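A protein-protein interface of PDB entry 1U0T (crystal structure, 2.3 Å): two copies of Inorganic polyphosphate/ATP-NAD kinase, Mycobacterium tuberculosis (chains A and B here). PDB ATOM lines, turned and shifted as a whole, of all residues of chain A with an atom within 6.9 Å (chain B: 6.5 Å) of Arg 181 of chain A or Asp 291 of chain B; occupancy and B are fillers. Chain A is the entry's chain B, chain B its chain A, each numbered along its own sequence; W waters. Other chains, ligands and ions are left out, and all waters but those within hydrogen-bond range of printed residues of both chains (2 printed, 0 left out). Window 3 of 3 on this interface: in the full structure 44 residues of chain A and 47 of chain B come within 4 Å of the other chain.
Water W1 bridges the side-chain carboxylate (OD1) of Asp 291 of chain B and the backbone carbonyl oxygen (O) of Pro 182 of chain A. Water W2 bridges the backbone carbonyl oxygen (O) of Asp 179 of chain A (3.2 Å) and the side-chain hydroxyl (OG1) of Thr 290 of chain B (3.3 Å).
No position is printed for both chains. Of the 15 pairs that touch across the chains among the printed residues, none has its exchanged pair printed and touching as well.
Of the printed residues of chain B, Val 175 of chain A touches Trp 304 (3.9 Å). Of the printed residues of chain B, Ile 178 of chain A touches Thr 290 (3.7 Å). Arg 181 of chain A touches three residues of chain B. Printed residues of chain B within 4 Å of Pro 182 of chain A: Thr 290, Val 294, Val 301 and Trp 304. Ala 242 of chain A touches none of the printed residues of chain B. Of the printed residues of chain A, Thr 290 of chain B touches Ile 178, Arg 181 and Pro 182. Asp 291 of chain B touches just one residue of chain A: Arg 181. Arg 292 of chain B touches none of the printed residues of chain A. The nearest residue of chain B that does not touch Arg 181 of chain A is Pro 288 of chain B (4.1 Å). The nearest residue of chain A that does not touch Asp 291 of chain B is Pro 182 of chain A (4.9 Å). The nearest printed residue of chain A that does not touch Thr 290 of chain B is Val 183 of chain A (4.05 Å).
Trp 304 of chain B touches Val 175 of chain A. Ile 178 of chain A touches Thr 290 of chain B (CB to OG1, 3.7 Å). CZ2 of Trp 304 of chain B touches O of Gly 180 of chain A, at 3.4 Å. NH1 of Arg 181 of chain A touches CZ3 of Trp 304 of chain B, at 3.5 Å. Pro 182 of chain A touches Thr 290 of chain B (O to CG2, 3.3 Å). Val 294 of chain B touches Pro 182 of chain A (CG2 to O, 3.4 Å). Pro 182 of chain A touches Val 301 of chain B. CD of Pro 182 of chain A touches CE2 of Trp 304 of chain B, at 3.6 Å. Val 183 of chain A touches Val 294 of chain B. Val 183 of chain A touches Val 301 of chain B (O to CG2, 3.4 Å).
The indole nitrogen of Trp 304 of chain B lies within hydrogen-bond range of the side-chain carboxylate of Glu 177 of chain A (2.8 Å). The guanidinium group (NE) of Arg 181 of chain A is in salt-bridge range of the side-chain carboxylate (OD1) of Asp 291 of chain B (3.0 Å).
Of the 12 printed residues of chain B, 6 touch a printed residue of chain A. Printed residues of chain B that touch a printed residue of chain A: Thr 290, Asp 291, Leu 293, Val 294, Val 301 and Trp 304. Of the 11 printed residues of chain A, 8 touch a printed residue of chain B. Hydrophobic or aromatic side chains of chain A within 4 Å of the printed part of chain B: Val 175, Ile 178, Pro 182 and Val 183. Among the printed residues, 15 pairs touch across the chains. Among the printed residues, Asp or Glu carboxylates within 4 Å of a Lys or Arg side-chain nitrogen of the other chain: Arg 181 of chain A with Asp 291 of chain B (3.0 Å).
The backbone NH of Val 183 of chain A is in hydrogen-bond range of the backbone carbonyl oxygen of Val 176 of chain A, 2.8 Å away. The backbone NH (N) of Val 176 of chain A sits at hydrogen-bond distance from the backbone carbonyl oxygen (O) of Ser 184 of chain A (2.8 Å). N of Glu 177 of chain A lies within hydrogen-bond range of O of Ala 242 of chain A.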
ATOM      1  N   VAL A 175       4.375  10.994  -4.121  1.00  0.00           N
ATOM      2  CA  VAL A 175       3.714  11.580  -5.272  1.00  0.00           C
ATOM      3  C   VAL A 175       2.671  10.533  -5.699  1.00  0.00           C
ATOM      4  O   VAL A 175       3.034   9.365  -5.888  1.00  0.00           O
ATOM      5  CB  VAL A 175       4.698  11.812  -6.464  1.00  0.00           C
ATOM      6  CG1 VAL A 175       3.982  12.427  -7.605  1.00  0.00           C
ATOM      7  CG2 VAL A 175       5.890  12.727  -6.054  1.00  0.00           C
ATOM      8  N   VAL A 176       1.403  10.945  -5.856  1.00  0.00           N
ATOM      9  CA  VAL A 176       0.351  10.083  -6.367  1.00  0.00           C
ATOM     10  C   VAL A 176       0.207  10.328  -7.877  1.00  0.00           C
ATOM     11  O   VAL A 176       0.157  11.463  -8.360  1.00  0.00           O
ATOM     12  CB  VAL A 176      -1.009  10.342  -5.622  1.00  0.00           C
ATOM     13  CG1 VAL A 176      -2.184   9.602  -6.308  1.00  0.00           C
ATOM     14  CG2 VAL A 176      -0.921   9.905  -4.204  1.00  0.00           C
ATOM     15  N   GLU A 177       0.178   9.257  -8.639  1.00  0.00           N
ATOM     16  CA  GLU A 177       0.203   9.360 -10.065  1.00  0.00           C
ATOM     17  C   GLU A 177      -0.981   8.535 -10.563  1.00  0.00           C
ATOM     18  O   GLU A 177      -1.174   7.383 -10.124  1.00  0.00           O
ATOM     19  CB  GLU A 177       1.525   8.817 -10.605  1.00  0.00           C
ATOM     20  CG  GLU A 177       1.529   8.514 -12.101  1.00  0.00           C
ATOM     21  CD  GLU A 177       2.685   7.606 -12.503  1.00  0.00           C
ATOM     22  OE1 GLU A 177       3.879   8.004 -12.335  1.00  0.00           O
ATOM     23  OE2 GLU A 177       2.398   6.496 -12.993  1.00  0.00           O
ATOM     24  N   ILE A 178      -1.798   9.103 -11.436  1.00  0.00           N
ATOM     25  CA  ILE A 178      -3.008   8.374 -11.743  1.00  0.00           C
ATOM     26  C   ILE A 178      -2.933   7.569 -13.026  1.00  0.00           C
ATOM     27  O   ILE A 178      -2.773   6.367 -12.949  1.00  0.00           O
ATOM     28  CB  ILE A 178      -4.290   9.189 -11.557  1.00  0.00           C
ATOM     29  CG1 ILE A 178      -4.565   9.397 -10.050  1.00  0.00           C
ATOM     30  CG2 ILE A 178      -5.491   8.472 -12.204  1.00  0.00           C
ATOM     31  CD1 ILE A 178      -4.219   8.245  -9.187  1.00  0.00           C
ATOM     32  N   ASP A 179      -3.015   8.148 -14.199  1.00  0.00           N
ATOM     33  CA  ASP A 179      -2.899   7.217 -15.345  1.00  0.00           C
ATOM     34  C   ASP A 179      -1.660   7.657 -16.101  1.00  0.00           C
ATOM     35  O   ASP A 179      -1.760   8.244 -17.166  1.00  0.00           O
ATOM     36  CB  ASP A 179      -4.129   7.272 -16.285  1.00  0.00           C
ATOM     37  CG  ASP A 179      -5.249   6.258 -15.912  1.00  0.00           C
ATOM     38  OD1 ASP A 179      -4.964   5.047 -15.700  1.00  0.00           O
ATOM     39  OD2 ASP A 179      -6.470   6.591 -15.857  1.00  0.00           O
ATOM     40  N   GLY A 180      -0.511   7.420 -15.507  1.00  0.00           N
ATOM     41  CA  GLY A 180       0.749   7.858 -16.101  1.00  0.00           C
ATOM     42  C   GLY A 180       1.139   9.309 -15.786  1.00  0.00           C
ATOM     43  O   GLY A 180       2.136   9.782 -16.294  1.00  0.00           O
ATOM     44  N   ARG A 181       0.344  10.015 -14.977  1.00  0.00           N
ATOM     45  CA  ARG A 181       0.523  11.457 -14.806  1.00  0.00           C
ATOM     46  C   ARG A 181       0.389  11.822 -13.339  1.00  0.00           C
ATOM     47  O   ARG A 181      -0.477  11.282 -12.654  1.00  0.00           O
ATOM     48  CB  ARG A 181      -0.486  12.257 -15.651  1.00  0.00           C
ATOM     49  CG  ARG A 181      -0.254  12.202 -17.175  1.00  0.00           C
ATOM     50  CD  ARG A 181       1.185  12.702 -17.622  1.00  0.00           C
ATOM     51  NE  ARG A 181       1.391  14.120 -17.348  1.00  0.00           N
ATOM     52  CZ  ARG A 181       2.541  14.781 -17.481  1.00  0.00           C
ATOM     53  NH1 ARG A 181       3.655  14.172 -17.876  1.00  0.00           N
ATOM     54  NH2 ARG A 181       2.576  16.073 -17.193  1.00  0.00           N
ATOM     55  N   PRO A 182       1.247  12.716 -12.847  1.00  0.00           N
ATOM     56  CA  PRO A 182       1.212  13.091 -11.433  1.00  0.00           C
ATOM     57  C   PRO A 182      -0.042  13.888 -11.103  1.00  0.00           C
ATOM     58  O   PRO A 182      -0.454  14.736 -11.896  1.00  0.00           O
ATOM     59  CB  PRO A 182       2.469  13.943 -11.270  1.00  0.00           C
ATOM     60  CG  PRO A 182       2.759  14.488 -12.655  1.00  0.00           C
ATOM     61  CD  PRO A 182       2.314  13.424 -13.593  1.00  0.00           C
ATOM     62  N   VAL A 183      -0.674  13.584  -9.963  1.00  0.00           N
ATOM     63  CA  VAL A 183      -1.822  14.370  -9.530  1.00  0.00           C
ATOM     64  C   VAL A 183      -1.512  15.228  -8.289  1.00  0.00           C
ATOM     65  O   VAL A 183      -1.922  16.365  -8.238  1.00  0.00           O
ATOM     66  CB  VAL A 183      -3.101  13.495  -9.338  1.00  0.00           C
ATOM     67  CG1 VAL A 183      -2.952  12.603  -8.141  1.00  0.00           C
ATOM     68  CG2 VAL A 183      -4.376  14.412  -9.172  1.00  0.00           C
ATOM     69  N   SER A 184      -0.793  14.695  -7.294  1.00  0.00           N
ATOM     70  CA  SER A 184      -0.404  15.498  -6.140  1.00  0.00           C
ATOM     71  C   SER A 184       0.841  14.949  -5.477  1.00  0.00           C
ATOM     72  O   SER A 184       1.049  13.745  -5.474  1.00  0.00           O
ATOM     73  CB  SER A 184      -1.543  15.561  -5.094  1.00  0.00           C
ATOM     74  OG  SER A 184      -2.515  16.515  -5.486  1.00  0.00           O
ATOM     75  N   ALA A 242      -0.409   4.850  -9.234  1.00  0.00           N
ATOM     76  CA  ALA A 242       0.955   4.610  -8.747  1.00  0.00           C
ATOM     77  C   ALA A 242       1.265   5.586  -7.634  1.00  0.00           C
ATOM     78  O   ALA A 242       0.903   6.764  -7.708  1.00  0.00           O
ATOM     79  CB  ALA A 242       1.938   4.777  -9.890  1.00  0.00           C
ATOM     80  N   ALA B 287      -5.068  17.051 -23.448  1.00  0.00           N
ATOM     81  CA  ALA B 287      -4.550  16.742 -22.109  1.00  0.00           C
ATOM     82  C   ALA B 287      -5.458  15.732 -21.387  1.00  0.00           C
ATOM     83  O   ALA B 287      -6.683  15.846 -21.438  1.00  0.00           O
ATOM     84  CB  ALA B 287      -4.414  18.016 -21.297  1.00  0.00           C
ATOM     85  N   PRO B 288      -4.907  14.717 -20.738  1.00  0.00           N
ATOM     86  CA  PRO B 288      -5.784  13.797 -20.012  1.00  0.00           C
ATOM     87  C   PRO B 288      -6.249  14.545 -18.750  1.00  0.00           C
ATOM     88  O   PRO B 288      -5.660  15.562 -18.347  1.00  0.00           O
ATOM     89  CB  PRO B 288      -4.868  12.644 -19.642  1.00  0.00           C
ATOM     90  CG  PRO B 288      -3.466  13.314 -19.481  1.00  0.00           C
ATOM     91  CD  PRO B 288      -3.478  14.376 -20.568  1.00  0.00           C
ATOM     92  N   PHE B 289      -7.327  14.042 -18.175  1.00  0.00           N
ATOM     93  CA  PHE B 289      -8.009  14.707 -17.092  1.00  0.00           C
ATOM     94  C   PHE B 289      -7.067  15.020 -15.920  1.00  0.00           C
ATOM     95  O   PHE B 289      -7.118  16.109 -15.387  1.00  0.00           O
ATOM     96  CB  PHE B 289      -9.189  13.858 -16.607  1.00  0.00           C
ATOM     97  CG  PHE B 289      -9.826  14.396 -15.353  1.00  0.00           C
ATOM     98  CD1 PHE B 289     -10.746  15.457 -15.426  1.00  0.00           C
ATOM     99  CD2 PHE B 289      -9.492  13.851 -14.099  1.00  0.00           C
ATOM    100  CE1 PHE B 289     -11.383  15.956 -14.232  1.00  0.00           C
ATOM    101  CE2 PHE B 289     -10.081  14.329 -12.888  1.00  0.00           C
ATOM    102  CZ  PHE B 289     -11.012  15.389 -12.930  1.00  0.00           C
ATOM    103  N   THR B 290      -6.232  14.075 -15.511  1.00  0.00           N
ATOM    104  CA  THR B 290      -5.279  14.353 -14.452  1.00  0.00           C
ATOM    105  C   THR B 290      -4.534  15.692 -14.687  1.00  0.00           C
ATOM    106  O   THR B 290      -4.338  16.467 -13.741  1.00  0.00           O
ATOM    107  CB  THR B 290      -4.231  13.245 -14.360  1.00  0.00           C
ATOM    108  OG1 THR B 290      -4.794  12.066 -13.781  1.00  0.00           O
ATOM    109  CG2 THR B 290      -3.175  13.634 -13.380  1.00  0.00           C
ATOM    110  N   ASP B 291      -4.102  15.958 -15.924  1.00  0.00           N
ATOM    111  CA  ASP B 291      -3.405  17.226 -16.195  1.00  0.00           C
ATOM    112  C   ASP B 291      -4.325  18.422 -16.105  1.00  0.00           C
ATOM    113  O   ASP B 291      -3.880  19.515 -15.751  1.00  0.00           O
ATOM    114  CB  ASP B 291      -2.734  17.242 -17.588  1.00  0.00           C
ATOM    115  CG  ASP B 291      -1.518  16.350 -17.670  1.00  0.00           C
ATOM    116  OD1 ASP B 291      -0.968  15.899 -16.645  1.00  0.00           O
ATOM    117  OD2 ASP B 291      -1.007  16.037 -18.744  1.00  0.00           O
ATOM    118  N   ARG B 292      -5.608  18.219 -16.417  1.00  0.00           N
ATOM    119  CA  ARG B 292      -6.588  19.309 -16.387  1.00  0.00           C
ATOM    120  C   ARG B 292      -6.893  19.656 -14.944  1.00  0.00           C
ATOM    121  O   ARG B 292      -7.024  20.832 -14.592  1.00  0.00           O
ATOM    122  CB  ARG B 292      -7.865  18.910 -17.095  1.00  0.00           C
ATOM    123  CG  ARG B 292      -7.712  18.582 -18.567  1.00  0.00           C
ATOM    124  CD  ARG B 292      -9.051  18.138 -19.211  1.00  0.00           C
ATOM    125  NE  ARG B 292      -8.827  17.473 -20.494  1.00  0.00           N
ATOM    126  CZ  ARG B 292      -9.635  17.541 -21.552  1.00  0.00           C
ATOM    127  NH1 ARG B 292     -10.774  18.245 -21.502  1.00  0.00           N
ATOM    128  NH2 ARG B 292      -9.311  16.876 -22.662  1.00  0.00           N
ATOM    129  N   LEU B 293      -6.975  18.619 -14.110  1.00  0.00           N
ATOM    130  CA  LEU B 293      -7.088  18.781 -12.658  1.00  0.00           C
ATOM    131  C   LEU B 293      -5.932  19.542 -12.025  1.00  0.00           C
ATOM    132  O   LEU B 293      -6.140  20.483 -11.270  1.00  0.00           O
ATOM    133  CB  LEU B 293      -7.193  17.410 -11.980  1.00  0.00           C
ATOM    134  CG  LEU B 293      -8.100  17.193 -10.781  1.00  0.00           C
ATOM    135  CD1 LEU B 293      -7.403  16.417  -9.690  1.00  0.00           C
ATOM    136  CD2 LEU B 293      -8.788  18.434 -10.282  1.00  0.00           C
ATOM    137  N   VAL B 294      -4.712  19.089 -12.284  1.00  0.00           N
ATOM    138  CA  VAL B 294      -3.529  19.717 -11.745  1.00  0.00           C
ATOM    139  C   VAL B 294      -3.473  21.196 -12.154  1.00  0.00           C
ATOM    140  O   VAL B 294      -3.286  22.091 -11.350  1.00  0.00           O
ATOM    141  CB  VAL B 294      -2.263  18.969 -12.260  1.00  0.00           C
ATOM    142  CG1 VAL B 294      -0.970  19.822 -12.055  1.00  0.00           C
ATOM    143  CG2 VAL B 294      -2.130  17.633 -11.567  1.00  0.00           C
ATOM    144  N   ARG B 295      -3.654  21.435 -13.432  1.00  0.00           N
ATOM    145  CA  ARG B 295      -3.647  22.777 -13.958  1.00  0.00           C
ATOM    146  C   ARG B 295      -4.723  23.644 -13.314  1.00  0.00           C
ATOM    147  O   ARG B 295      -4.429  24.767 -12.840  1.00  0.00           O
ATOM    148  CB  ARG B 295      -3.895  22.681 -15.448  1.00  0.00           C
ATOM    149  CG  ARG B 295      -4.199  23.993 -16.150  1.00  0.00           C
ATOM    150  CD  ARG B 295      -3.604  23.998 -17.573  1.00  0.00           C
ATOM    151  NE  ARG B 295      -3.620  25.310 -18.228  1.00  0.00           N
ATOM    152  CZ  ARG B 295      -3.967  25.505 -19.497  1.00  0.00           C
ATOM    153  NH1 ARG B 295      -4.381  24.488 -20.259  1.00  0.00           N
ATOM    154  NH2 ARG B 295      -3.924  26.729 -20.001  1.00  0.00           N
ATOM    155  N   LYS B 296      -5.967  23.138 -13.294  1.00  0.00           N
ATOM    156  CA  LYS B 296      -7.079  23.960 -12.790  1.00  0.00           C
ATOM    157  C   LYS B 296      -6.874  24.390 -11.334  1.00  0.00           C
ATOM    158  O   LYS B 296      -7.094  25.547 -10.998  1.00  0.00           O
ATOM    159  CB  LYS B 296      -8.456  23.282 -12.954  1.00  0.00           C
ATOM    160  CG  LYS B 296      -9.687  24.163 -12.445  1.00  0.00           C
ATOM    161  CD  LYS B 296     -10.117  25.191 -13.514  1.00  0.00           C
ATOM    162  CE  LYS B 296     -11.542  25.751 -13.268  1.00  0.00           C
ATOM    163  NZ  LYS B 296     -11.582  26.520 -11.997  1.00  0.00           N
ATOM    164  N   VAL B 301       2.943  19.237  -7.799  1.00  0.00           N
ATOM    165  CA  VAL B 301       3.346  17.949  -8.363  1.00  0.00           C
ATOM    166  C   VAL B 301       4.882  17.759  -8.477  1.00  0.00           C
ATOM    167  O   VAL B 301       5.371  16.890  -9.226  1.00  0.00           O
ATOM    168  CB  VAL B 301       2.618  17.723  -9.708  1.00  0.00           C
ATOM    169  CG1 VAL B 301       3.358  16.781 -10.551  1.00  0.00           C
ATOM    170  CG2 VAL B 301       1.135  17.200  -9.482  1.00  0.00           C
ATOM    171  N   TRP B 304       7.987  14.345  -8.965  1.00  0.00           N
ATOM    172  CA  TRP B 304       7.512  13.217  -9.777  1.00  0.00           C
ATOM    173  C   TRP B 304       8.650  12.576 -10.559  1.00  0.00           C
ATOM    174  O   TRP B 304       9.299  13.255 -11.338  1.00  0.00           O
ATOM    175  CB  TRP B 304       6.446  13.689 -10.792  1.00  0.00           C
ATOM    176  CG  TRP B 304       5.864  12.570 -11.624  1.00  0.00           C
ATOM    177  CD1 TRP B 304       5.359  11.393 -11.159  1.00  0.00           C
ATOM    178  CD2 TRP B 304       5.753  12.514 -13.046  1.00  0.00           C
ATOM    179  NE1 TRP B 304       4.907  10.619 -12.197  1.00  0.00           N
ATOM    180  CE2 TRP B 304       5.157  11.275 -13.372  1.00  0.00           C
ATOM    181  CE3 TRP B 304       6.100  13.389 -14.091  1.00  0.00           C
ATOM    182  CZ2 TRP B 304       4.887  10.887 -14.695  1.00  0.00           C
ATOM    183  CZ3 TRP B 304       5.836  13.010 -15.391  1.00  0.00           C
ATOM    184  CH2 TRP B 304       5.243  11.763 -15.688  1.00  0.00           C
HETATM  185  O   HOH W   1      -0.167  16.272 -14.146  1.00  0.00           O
HETATM  186  O   HOH W   2      -3.465  10.849 -16.563  1.00  0.00           O
